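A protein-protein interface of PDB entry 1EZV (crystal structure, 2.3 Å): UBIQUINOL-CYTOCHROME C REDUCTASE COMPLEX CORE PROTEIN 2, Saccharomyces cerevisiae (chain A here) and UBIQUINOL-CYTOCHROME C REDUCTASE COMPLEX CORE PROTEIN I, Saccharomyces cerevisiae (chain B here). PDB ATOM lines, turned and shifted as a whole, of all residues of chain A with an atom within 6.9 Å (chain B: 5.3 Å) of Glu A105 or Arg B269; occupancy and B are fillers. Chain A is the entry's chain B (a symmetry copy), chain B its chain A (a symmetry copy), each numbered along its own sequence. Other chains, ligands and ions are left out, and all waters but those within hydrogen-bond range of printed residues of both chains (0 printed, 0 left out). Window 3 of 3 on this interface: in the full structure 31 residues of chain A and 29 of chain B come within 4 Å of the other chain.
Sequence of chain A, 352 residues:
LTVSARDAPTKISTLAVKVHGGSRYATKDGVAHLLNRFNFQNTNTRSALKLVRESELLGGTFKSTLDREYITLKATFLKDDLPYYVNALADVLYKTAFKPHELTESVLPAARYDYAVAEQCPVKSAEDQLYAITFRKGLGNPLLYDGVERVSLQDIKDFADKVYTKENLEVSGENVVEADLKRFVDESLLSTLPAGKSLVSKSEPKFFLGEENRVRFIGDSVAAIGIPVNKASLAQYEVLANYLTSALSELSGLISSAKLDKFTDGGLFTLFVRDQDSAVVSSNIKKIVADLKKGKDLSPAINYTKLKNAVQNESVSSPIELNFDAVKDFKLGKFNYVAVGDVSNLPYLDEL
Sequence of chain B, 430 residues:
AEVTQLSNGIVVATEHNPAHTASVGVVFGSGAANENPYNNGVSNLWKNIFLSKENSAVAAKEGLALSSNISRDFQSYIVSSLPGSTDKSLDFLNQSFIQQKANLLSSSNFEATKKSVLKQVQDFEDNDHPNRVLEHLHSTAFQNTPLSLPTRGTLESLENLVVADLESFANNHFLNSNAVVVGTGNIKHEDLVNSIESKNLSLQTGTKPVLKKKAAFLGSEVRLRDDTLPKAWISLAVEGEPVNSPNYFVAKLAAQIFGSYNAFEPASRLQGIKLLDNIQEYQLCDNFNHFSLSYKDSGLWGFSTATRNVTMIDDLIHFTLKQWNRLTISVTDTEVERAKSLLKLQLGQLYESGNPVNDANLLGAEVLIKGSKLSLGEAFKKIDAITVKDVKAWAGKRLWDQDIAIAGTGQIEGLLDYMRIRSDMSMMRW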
ATOM      1  N   LEU A  49       8.111  22.037  24.048  1.00  0.00           N
ATOM      2  CA  LEU A  49       9.565  22.023  24.180  1.00  0.00           C
ATOM      3  C   LEU A  49      10.127  23.387  24.598  1.00  0.00           C
ATOM      4  O   LEU A  49      10.870  23.481  25.579  1.00  0.00           O
ATOM      5  CB  LEU A  49      10.210  21.556  22.864  1.00  0.00           C
ATOM      6  CG  LEU A  49      11.722  21.729  22.706  1.00  0.00           C
ATOM      7  CD1 LEU A  49      12.465  20.816  23.663  1.00  0.00           C
ATOM      8  CD2 LEU A  49      12.110  21.426  21.272  1.00  0.00           C
ATOM      9  N   VAL A  52       9.348  24.549  28.256  1.00  0.00           N
ATOM     10  CA  VAL A  52      10.268  23.918  29.193  1.00  0.00           C
ATOM     11  C   VAL A  52      11.657  24.552  29.114  1.00  0.00           C
ATOM     12  O   VAL A  52      12.234  24.937  30.129  1.00  0.00           O
ATOM     13  CB  VAL A  52      10.373  22.392  28.926  1.00  0.00           C
ATOM     14  CG1 VAL A  52      11.434  21.762  29.820  1.00  0.00           C
ATOM     15  CG2 VAL A  52       9.027  21.726  29.159  1.00  0.00           C
ATOM     16  N   ARG A  53      12.181  24.712  27.909  1.00  0.00           N
ATOM     17  CA  ARG A  53      13.538  25.223  27.777  1.00  0.00           C
ATOM     18  C   ARG A  53      13.643  26.658  28.278  1.00  0.00           C
ATOM     19  O   ARG A  53      14.630  27.018  28.915  1.00  0.00           O
ATOM     20  CB  ARG A  53      14.018  25.125  26.326  1.00  0.00           C
ATOM     21  CG  ARG A  53      13.790  23.756  25.701  1.00  0.00           C
ATOM     22  CD  ARG A  53      14.439  22.645  26.517  1.00  0.00           C
ATOM     23  NE  ARG A  53      15.835  22.482  26.149  1.00  0.00           N
ATOM     24  CZ  ARG A  53      16.274  21.611  25.244  1.00  0.00           C
ATOM     25  NH1 ARG A  53      17.488  21.759  24.741  1.00  0.00           N
ATOM     26  NH2 ARG A  53      15.570  20.525  24.958  1.00  0.00           N
ATOM     27  N   PRO A 100      -3.696  16.188  16.764  1.00  0.00           N
ATOM     28  CA  PRO A 100      -4.030  14.756  16.846  1.00  0.00           C
ATOM     29  C   PRO A 100      -2.841  13.866  17.225  1.00  0.00           C
ATOM     30  O   PRO A 100      -3.014  12.827  17.862  1.00  0.00           O
ATOM     31  CB  PRO A 100      -4.550  14.419  15.442  1.00  0.00           C
ATOM     32  CG  PRO A 100      -4.937  15.733  14.851  1.00  0.00           C
ATOM     33  CD  PRO A 100      -3.966  16.729  15.421  1.00  0.00           C
ATOM     34  N   HIS A 101      -1.638  14.276  16.832  1.00  0.00           N
ATOM     35  CA  HIS A 101      -0.449  13.477  17.086  1.00  0.00           C
ATOM     36  C   HIS A 101       0.066  13.654  18.509  1.00  0.00           C
ATOM     37  O   HIS A 101       0.791  12.801  19.020  1.00  0.00           O
ATOM     38  CB  HIS A 101       0.652  13.809  16.075  1.00  0.00           C
ATOM     39  CG  HIS A 101       1.286  15.151  16.273  1.00  0.00           C
ATOM     40  ND1 HIS A 101       1.044  16.216  15.434  1.00  0.00           N
ATOM     41  CD2 HIS A 101       2.240  15.567  17.142  1.00  0.00           C
ATOM     42  CE1 HIS A 101       1.829  17.226  15.769  1.00  0.00           C
ATOM     43  NE2 HIS A 101       2.562  16.859  16.803  1.00  0.00           N
ATOM     44  N   GLU A 102      -0.258  14.793  19.119  1.00  0.00           N
ATOM     45  CA  GLU A 102       0.050  15.020  20.529  1.00  0.00           C
ATOM     46  C   GLU A 102      -0.807  14.106  21.384  1.00  0.00           C
ATOM     47  O   GLU A 102      -0.363  13.612  22.417  1.00  0.00           O
ATOM     48  CB  GLU A 102      -0.219  16.467  20.914  1.00  0.00           C
ATOM     49  CG  GLU A 102       0.643  17.458  20.180  1.00  0.00           C
ATOM     50  CD  GLU A 102       0.547  18.839  20.771  1.00  0.00           C
ATOM     51  OE1 GLU A 102      -0.437  19.547  20.465  1.00  0.00           O
ATOM     52  OE2 GLU A 102       1.444  19.205  21.558  1.00  0.00           O
ATOM     53  N   LEU A 103      -2.020  13.842  20.913  1.00  0.00           N
ATOM     54  CA  LEU A 103      -2.900  12.905  21.585  1.00  0.00           C
ATOM     55  C   LEU A 103      -2.241  11.529  21.643  1.00  0.00           C
ATOM     56  O   LEU A 103      -1.932  11.032  22.731  1.00  0.00           O
ATOM     57  CB  LEU A 103      -4.247  12.819  20.860  1.00  0.00           C
ATOM     58  CG  LEU A 103      -5.288  11.895  21.498  1.00  0.00           C
ATOM     59  CD1 LEU A 103      -5.465  12.260  22.969  1.00  0.00           C
ATOM     60  CD2 LEU A 103      -6.608  11.993  20.743  1.00  0.00           C
ATOM     61  N   THR A 104      -1.884  11.005  20.470  1.00  0.00           N
ATOM     62  CA  THR A 104      -1.398   9.630  20.343  1.00  0.00           C
ATOM     63  C   THR A 104       0.020   9.406  20.877  1.00  0.00           C
ATOM     64  O   THR A 104       0.328   8.329  21.384  1.00  0.00           O
ATOM     65  CB  THR A 104      -1.451   9.150  18.876  1.00  0.00           C
ATOM     66  OG1 THR A 104      -0.627   9.995  18.069  1.00  0.00           O
ATOM     67  CG2 THR A 104      -2.873   9.195  18.347  1.00  0.00           C
ATOM     68  N   GLU A 105       0.853  10.440  20.828  1.00  0.00           N
ATOM     69  CA  GLU A 105       2.266  10.303  21.171  1.00  0.00           C
ATOM     70  C   GLU A 105       2.625  10.684  22.601  1.00  0.00           C
ATOM     71  O   GLU A 105       3.649  10.233  23.111  1.00  0.00           O
ATOM     72  CB  GLU A 105       3.130  11.126  20.213  1.00  0.00           C
ATOM     73  CG  GLU A 105       3.115  10.633  18.781  1.00  0.00           C
ATOM     74  CD  GLU A 105       3.919  11.514  17.842  1.00  0.00           C
ATOM     75  OE1 GLU A 105       4.678  12.390  18.325  1.00  0.00           O
ATOM     76  OE2 GLU A 105       3.787  11.331  16.614  1.00  0.00           O
ATOM     77  N   SER A 106       1.839  11.564  23.221  1.00  0.00           N
ATOM     78  CA  SER A 106       2.189  12.091  24.542  1.00  0.00           C
ATOM     79  C   SER A 106       1.102  11.961  25.597  1.00  0.00           C
ATOM     80  O   SER A 106       1.400  11.698  26.761  1.00  0.00           O
ATOM     81  CB  SER A 106       2.602  13.559  24.445  1.00  0.00           C
ATOM     82  OG  SER A 106       3.811  13.696  23.722  1.00  0.00           O
ATOM     83  N   VAL A 107      -0.144  12.209  25.202  1.00  0.00           N
ATOM     84  CA  VAL A 107      -1.246  12.328  26.153  1.00  0.00           C
ATOM     85  C   VAL A 107      -1.824  10.967  26.531  1.00  0.00           C
ATOM     86  O   VAL A 107      -1.961  10.653  27.717  1.00  0.00           O
ATOM     87  CB  VAL A 107      -2.365  13.256  25.592  1.00  0.00           C
ATOM     88  CG1 VAL A 107      -3.621  13.183  26.460  1.00  0.00           C
ATOM     89  CG2 VAL A 107      -1.859  14.691  25.536  1.00  0.00           C
ATOM     90  N   LEU A 108      -2.105  10.141  25.529  1.00  0.00           N
ATOM     91  CA  LEU A 108      -2.610   8.792  25.769  1.00  0.00           C
ATOM     92  C   LEU A 108      -1.613   7.877  26.500  1.00  0.00           C
ATOM     93  O   LEU A 108      -1.993   7.182  27.436  1.00  0.00           O
ATOM     94  CB  LEU A 108      -3.056   8.144  24.454  1.00  0.00           C
ATOM     95  CG  LEU A 108      -4.380   8.636  23.870  1.00  0.00           C
ATOM     96  CD1 LEU A 108      -4.699   7.882  22.581  1.00  0.00           C
ATOM     97  CD2 LEU A 108      -5.493   8.436  24.896  1.00  0.00           C
ATOM     98  N   PRO A 109      -0.325   7.881  26.096  1.00  0.00           N
ATOM     99  CA  PRO A 109       0.699   7.201  26.900  1.00  0.00           C
ATOM    100  C   PRO A 109       0.750   7.649  28.354  1.00  0.00           C
ATOM    101  O   PRO A 109       0.720   6.819  29.261  1.00  0.00           O
ATOM    102  CB  PRO A 109       1.998   7.525  26.164  1.00  0.00           C
ATOM    103  CG  PRO A 109       1.571   7.585  24.748  1.00  0.00           C
ATOM    104  CD  PRO A 109       0.203   8.236  24.762  1.00  0.00           C
ATOM    105  N   ALA A 110       0.821   8.960  28.572  1.00  0.00           N
ATOM    106  CA  ALA A 110       0.938   9.506  29.923  1.00  0.00           C
ATOM    107  C   ALA A 110      -0.272   9.157  30.780  1.00  0.00           C
ATOM    108  O   ALA A 110      -0.129   8.847  31.958  1.00  0.00           O
ATOM    109  CB  ALA A 110       1.127  11.010  29.869  1.00  0.00           C
ATOM    110  N   TYR B 261      15.227  12.531  35.989  1.00  0.00           N
ATOM    111  CA  TYR B 261      14.458  12.184  34.807  1.00  0.00           C
ATOM    112  C   TYR B 261      13.419  11.112  35.095  1.00  0.00           C
ATOM    113  O   TYR B 261      13.626  10.241  35.929  1.00  0.00           O
ATOM    114  CB  TYR B 261      15.412  11.731  33.694  1.00  0.00           C
ATOM    115  CG  TYR B 261      14.750  11.057  32.512  1.00  0.00           C
ATOM    116  CD1 TYR B 261      14.785   9.670  32.370  1.00  0.00           C
ATOM    117  CD2 TYR B 261      14.129  11.805  31.514  1.00  0.00           C
ATOM    118  CE1 TYR B 261      14.220   9.043  31.262  1.00  0.00           C
ATOM    119  CE2 TYR B 261      13.569  11.186  30.397  1.00  0.00           C
ATOM    120  CZ  TYR B 261      13.620   9.805  30.283  1.00  0.00           C
ATOM    121  OH  TYR B 261      13.051   9.183  29.195  1.00  0.00           O
ATOM    122  N   ASN B 262      12.314  11.175  34.364  1.00  0.00           N
ATOM    123  CA  ASN B 262      11.221  10.226  34.497  1.00  0.00           C
ATOM    124  C   ASN B 262      10.647  10.044  33.093  1.00  0.00           C
ATOM    125  O   ASN B 262       9.998  10.943  32.556  1.00  0.00           O
ATOM    126  CB  ASN B 262      10.155  10.794  35.444  1.00  0.00           C
ATOM    127  CG  ASN B 262       9.022   9.806  35.741  1.00  0.00           C
ATOM    128  OD1 ASN B 262       8.386   9.895  36.793  1.00  0.00           O
ATOM    129  ND2 ASN B 262       8.725   8.909  34.796  1.00  0.00           N
ATOM    130  N   ALA B 263      10.857   8.859  32.531  1.00  0.00           N
ATOM    131  CA  ALA B 263      10.506   8.564  31.148  1.00  0.00           C
ATOM    132  C   ALA B 263       9.024   8.694  30.845  1.00  0.00           C
ATOM    133  O   ALA B 263       8.636   8.813  29.686  1.00  0.00           O
ATOM    134  CB  ALA B 263      10.981   7.167  30.787  1.00  0.00           C
ATOM    135  N   PHE B 264       8.184   8.608  31.869  1.00  0.00           N
ATOM    136  CA  PHE B 264       6.740   8.596  31.637  1.00  0.00           C
ATOM    137  C   PHE B 264       6.084   9.980  31.733  1.00  0.00           C
ATOM    138  O   PHE B 264       4.967  10.177  31.244  1.00  0.00           O
ATOM    139  CB  PHE B 264       6.071   7.605  32.591  1.00  0.00           C
ATOM    140  CG  PHE B 264       6.581   6.196  32.446  1.00  0.00           C
ATOM    141  CD1 PHE B 264       7.638   5.741  33.227  1.00  0.00           C
ATOM    142  CD2 PHE B 264       6.058   5.350  31.473  1.00  0.00           C
ATOM    143  CE1 PHE B 264       8.173   4.463  33.037  1.00  0.00           C
ATOM    144  CE2 PHE B 264       6.589   4.072  31.274  1.00  0.00           C
ATOM    145  CZ  PHE B 264       7.650   3.628  32.059  1.00  0.00           C
ATOM    146  N   GLU B 265       6.828  10.947  32.272  1.00  0.00           N
ATOM    147  CA  GLU B 265       6.384  12.338  32.357  1.00  0.00           C
ATOM    148  C   GLU B 265       6.813  13.133  31.118  1.00  0.00           C
ATOM    149  O   GLU B 265       7.989  13.476  30.966  1.00  0.00           O
ATOM    150  CB  GLU B 265       6.956  13.008  33.621  1.00  0.00           C
ATOM    151  CG  GLU B 265       6.229  12.663  34.920  1.00  0.00           C
ATOM    152  CD  GLU B 265       4.753  13.059  34.907  1.00  0.00           C
ATOM    153  OE1 GLU B 265       3.910  12.246  35.346  1.00  0.00           O
ATOM    154  OE2 GLU B 265       4.435  14.181  34.451  1.00  0.00           O
ATOM    155  N   PRO B 266       5.853  13.469  30.240  1.00  0.00           N
ATOM    156  CA  PRO B 266       6.097  14.202  28.990  1.00  0.00           C
ATOM    157  C   PRO B 266       7.057  15.384  29.130  1.00  0.00           C
ATOM    158  O   PRO B 266       8.014  15.518  28.360  1.00  0.00           O
ATOM    159  CB  PRO B 266       4.701  14.650  28.576  1.00  0.00           C
ATOM    160  CG  PRO B 266       3.821  13.535  29.068  1.00  0.00           C
ATOM    161  CD  PRO B 266       4.421  13.145  30.402  1.00  0.00           C
ATOM    162  N   ALA B 267       6.857  16.174  30.180  1.00  0.00           N
ATOM    163  CA  ALA B 267       7.693  17.345  30.430  1.00  0.00           C
ATOM    164  C   ALA B 267       9.139  16.968  30.691  1.00  0.00           C
ATOM    165  O   ALA B 267      10.046  17.747  30.401  1.00  0.00           O
ATOM    166  CB  ALA B 267       7.148  18.140  31.617  1.00  0.00           C
ATOM    167  N   SER B 268       9.348  15.820  31.330  1.00  0.00           N
ATOM    168  CA  SER B 268      10.693  15.401  31.729  1.00  0.00           C
ATOM    169  C   SER B 268      11.552  15.052  30.516  1.00  0.00           C
ATOM    170  O   SER B 268      12.749  15.342  30.491  1.00  0.00           O
ATOM    171  CB  SER B 268      10.620  14.199  32.675  1.00  0.00           C
ATOM    172  OG  SER B 268      11.828  14.052  33.405  1.00  0.00           O
ATOM    173  N   ARG B 269      10.905  14.531  29.478  1.00  0.00           N
ATOM    174  CA  ARG B 269      11.582  14.147  28.243  1.00  0.00           C
ATOM    175  C   ARG B 269      12.076  15.364  27.462  1.00  0.00           C
ATOM    176  O   ARG B 269      12.785  15.219  26.463  1.00  0.00           O
ATOM    177  CB  ARG B 269      10.638  13.322  27.359  1.00  0.00           C
ATOM    178  CG  ARG B 269       9.828  12.272  28.112  1.00  0.00           C
ATOM    179  CD  ARG B 269       9.477  11.085  27.231  1.00  0.00           C
ATOM    180  NE  ARG B 269       8.296  11.333  26.412  1.00  0.00           N
ATOM    181  CZ  ARG B 269       7.231  10.532  26.359  1.00  0.00           C
ATOM    182  NH1 ARG B 269       6.189  10.855  25.593  1.00  0.00           N
ATOM    183  NH2 ARG B 269       7.198   9.405  27.068  1.00  0.00           N
ATOM    184  N   LEU B 270      11.687  16.561  27.902  1.00  0.00           N
ATOM    185  CA  LEU B 270      11.952  17.774  27.132  1.00  0.00           C
ATOM    186  C   LEU B 270      13.012  18.676  27.759  1.00  0.00           C
ATOM    187  O   LEU B 270      13.409  19.677  27.168  1.00  0.00           O
ATOM    188  CB  LEU B 270      10.658  18.558  26.924  1.00  0.00           C
ATOM    189  CG  LEU B 270       9.490  17.814  26.270  1.00  0.00           C
ATOM    190  CD1 LEU B 270       8.217  18.673  26.343  1.00  0.00           C
ATOM    191  CD2 LEU B 270       9.832  17.477  24.823  1.00  0.00           C
ATOM    192  N   GLN B 271      13.530  18.285  28.915  1.00  0.00           N
ATOM    193  CA  GLN B 271      14.533  19.095  29.592  1.00  0.00           C
ATOM    194  C   GLN B 271      15.795  19.349  28.773  1.00  0.00           C
ATOM    195  O   GLN B 271      16.231  18.491  27.986  1.00  0.00           O
ATOM    196  CB  GLN B 271      14.925  18.448  30.914  1.00  0.00           C
ATOM    197  CG  GLN B 271      13.770  18.206  31.853  1.00  0.00           C
ATOM    198  CD  GLN B 271      14.210  17.449  33.076  1.00  0.00           C
ATOM    199  OE1 GLN B 271      15.034  17.941  33.851  1.00  0.00           O
ATOM    200  NE2 GLN B 271      13.789  16.191  33.176  1.00  0.00           N
ATOM    201  N   LEU B 276      19.837  13.175  27.492  1.00  0.00           N
ATOM    202  CA  LEU B 276      18.517  12.652  27.130  1.00  0.00           C
ATOM    203  C   LEU B 276      18.392  12.280  25.661  1.00  0.00           C
ATOM    204  O   LEU B 276      17.526  11.483  25.293  1.00  0.00           O
ATOM    205  CB  LEU B 276      17.420  13.655  27.482  1.00  0.00           C
ATOM    206  CG  LEU B 276      17.145  13.890  28.964  1.00  0.00           C
ATOM    207  CD1 LEU B 276      15.841  14.663  29.089  1.00  0.00           C
ATOM    208  CD2 LEU B 276      17.058  12.566  29.719  1.00  0.00           C
ATOM    209  N   GLN B 280      17.051   8.181  25.276  1.00  0.00           N
ATOM    210  CA  GLN B 280      15.649   8.054  24.883  1.00  0.00           C
ATOM    211  C   GLN B 280      15.429   7.258  23.607  1.00  0.00           C
ATOM    212  O   GLN B 280      14.348   6.706  23.402  1.00  0.00           O
ATOM    213  CB  GLN B 280      15.007   9.429  24.747  1.00  0.00           C
ATOM    214  CG  GLN B 280      14.887  10.164  26.066  1.00  0.00           C
ATOM    215  CD  GLN B 280      13.819  11.229  26.035  1.00  0.00           C
ATOM    216  OE1 GLN B 280      12.653  10.958  26.331  1.00  0.00           O
ATOM    217  NE2 GLN B 280      14.195  12.433  25.618  1.00  0.00           N
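Printed residues of chain B within 4 Å of Leu A49: Leu B270 (3.8 Å). Printed residues of chain B within 4 Å of Arg A53: Leu B270 (3.2 Å) and Gln B271 (3.7 Å). Of chain B, only Arg B269 (3.6 Å) comes within 4 Å of Glu A105. Printed residues of chain B within 4 Å of Ser A106: Pro B266. Of chain A, only Glu A105 comes within 4 Å of Arg B269. Printed residues of chain A within 4 Å of Leu B270: Leu A49 (3.8 Å), Val A52 (3.9 Å) and Arg A53 (3.2 Å). The nearest printed residue of chain A that does not touch Leu B270 is Ser A106 (7.1 Å).
The backbone carbonyl oxygen (O) of Ala B263 lies within hydrogen-bond range of the guanidinium group (NH2) of Arg B269, at 3.0 Å. OG of Ser B268 sits at hydrogen-bond distance from NE2 of Gln B271, at 2.9 Å. NE2 of Gln B280 lies within hydrogen-bond range of O of Arg B269 (3.2 Å).
O of Leu B270 touches CD1 of Leu A49, 3.8 Å away. Val A52 touches Leu B270 (CG1 to O, 3.9 Å). Arg A53 touches Gln B271. Glu A105 touches Arg B269. Pro B266 touches Ser A106. Ala A110 touches Pro B266 (CB to CG, 3.8 Å).
NH2 of Arg A53 is in hydrogen-bond range of O of Leu B270.
Of the 14 printed residues of chain A, 6 touch a printed residue of chain B. Of the 13 printed residues of chain B, 4 touch a printed residue of chain A. Along chain B the printed residues that touch a printed residue of chain A span positions 266 to 271. Among the printed residues, no Asp or Glu carboxylate lies within 4 Å of a Lys or Arg side-chain nitrogen of the other chain.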
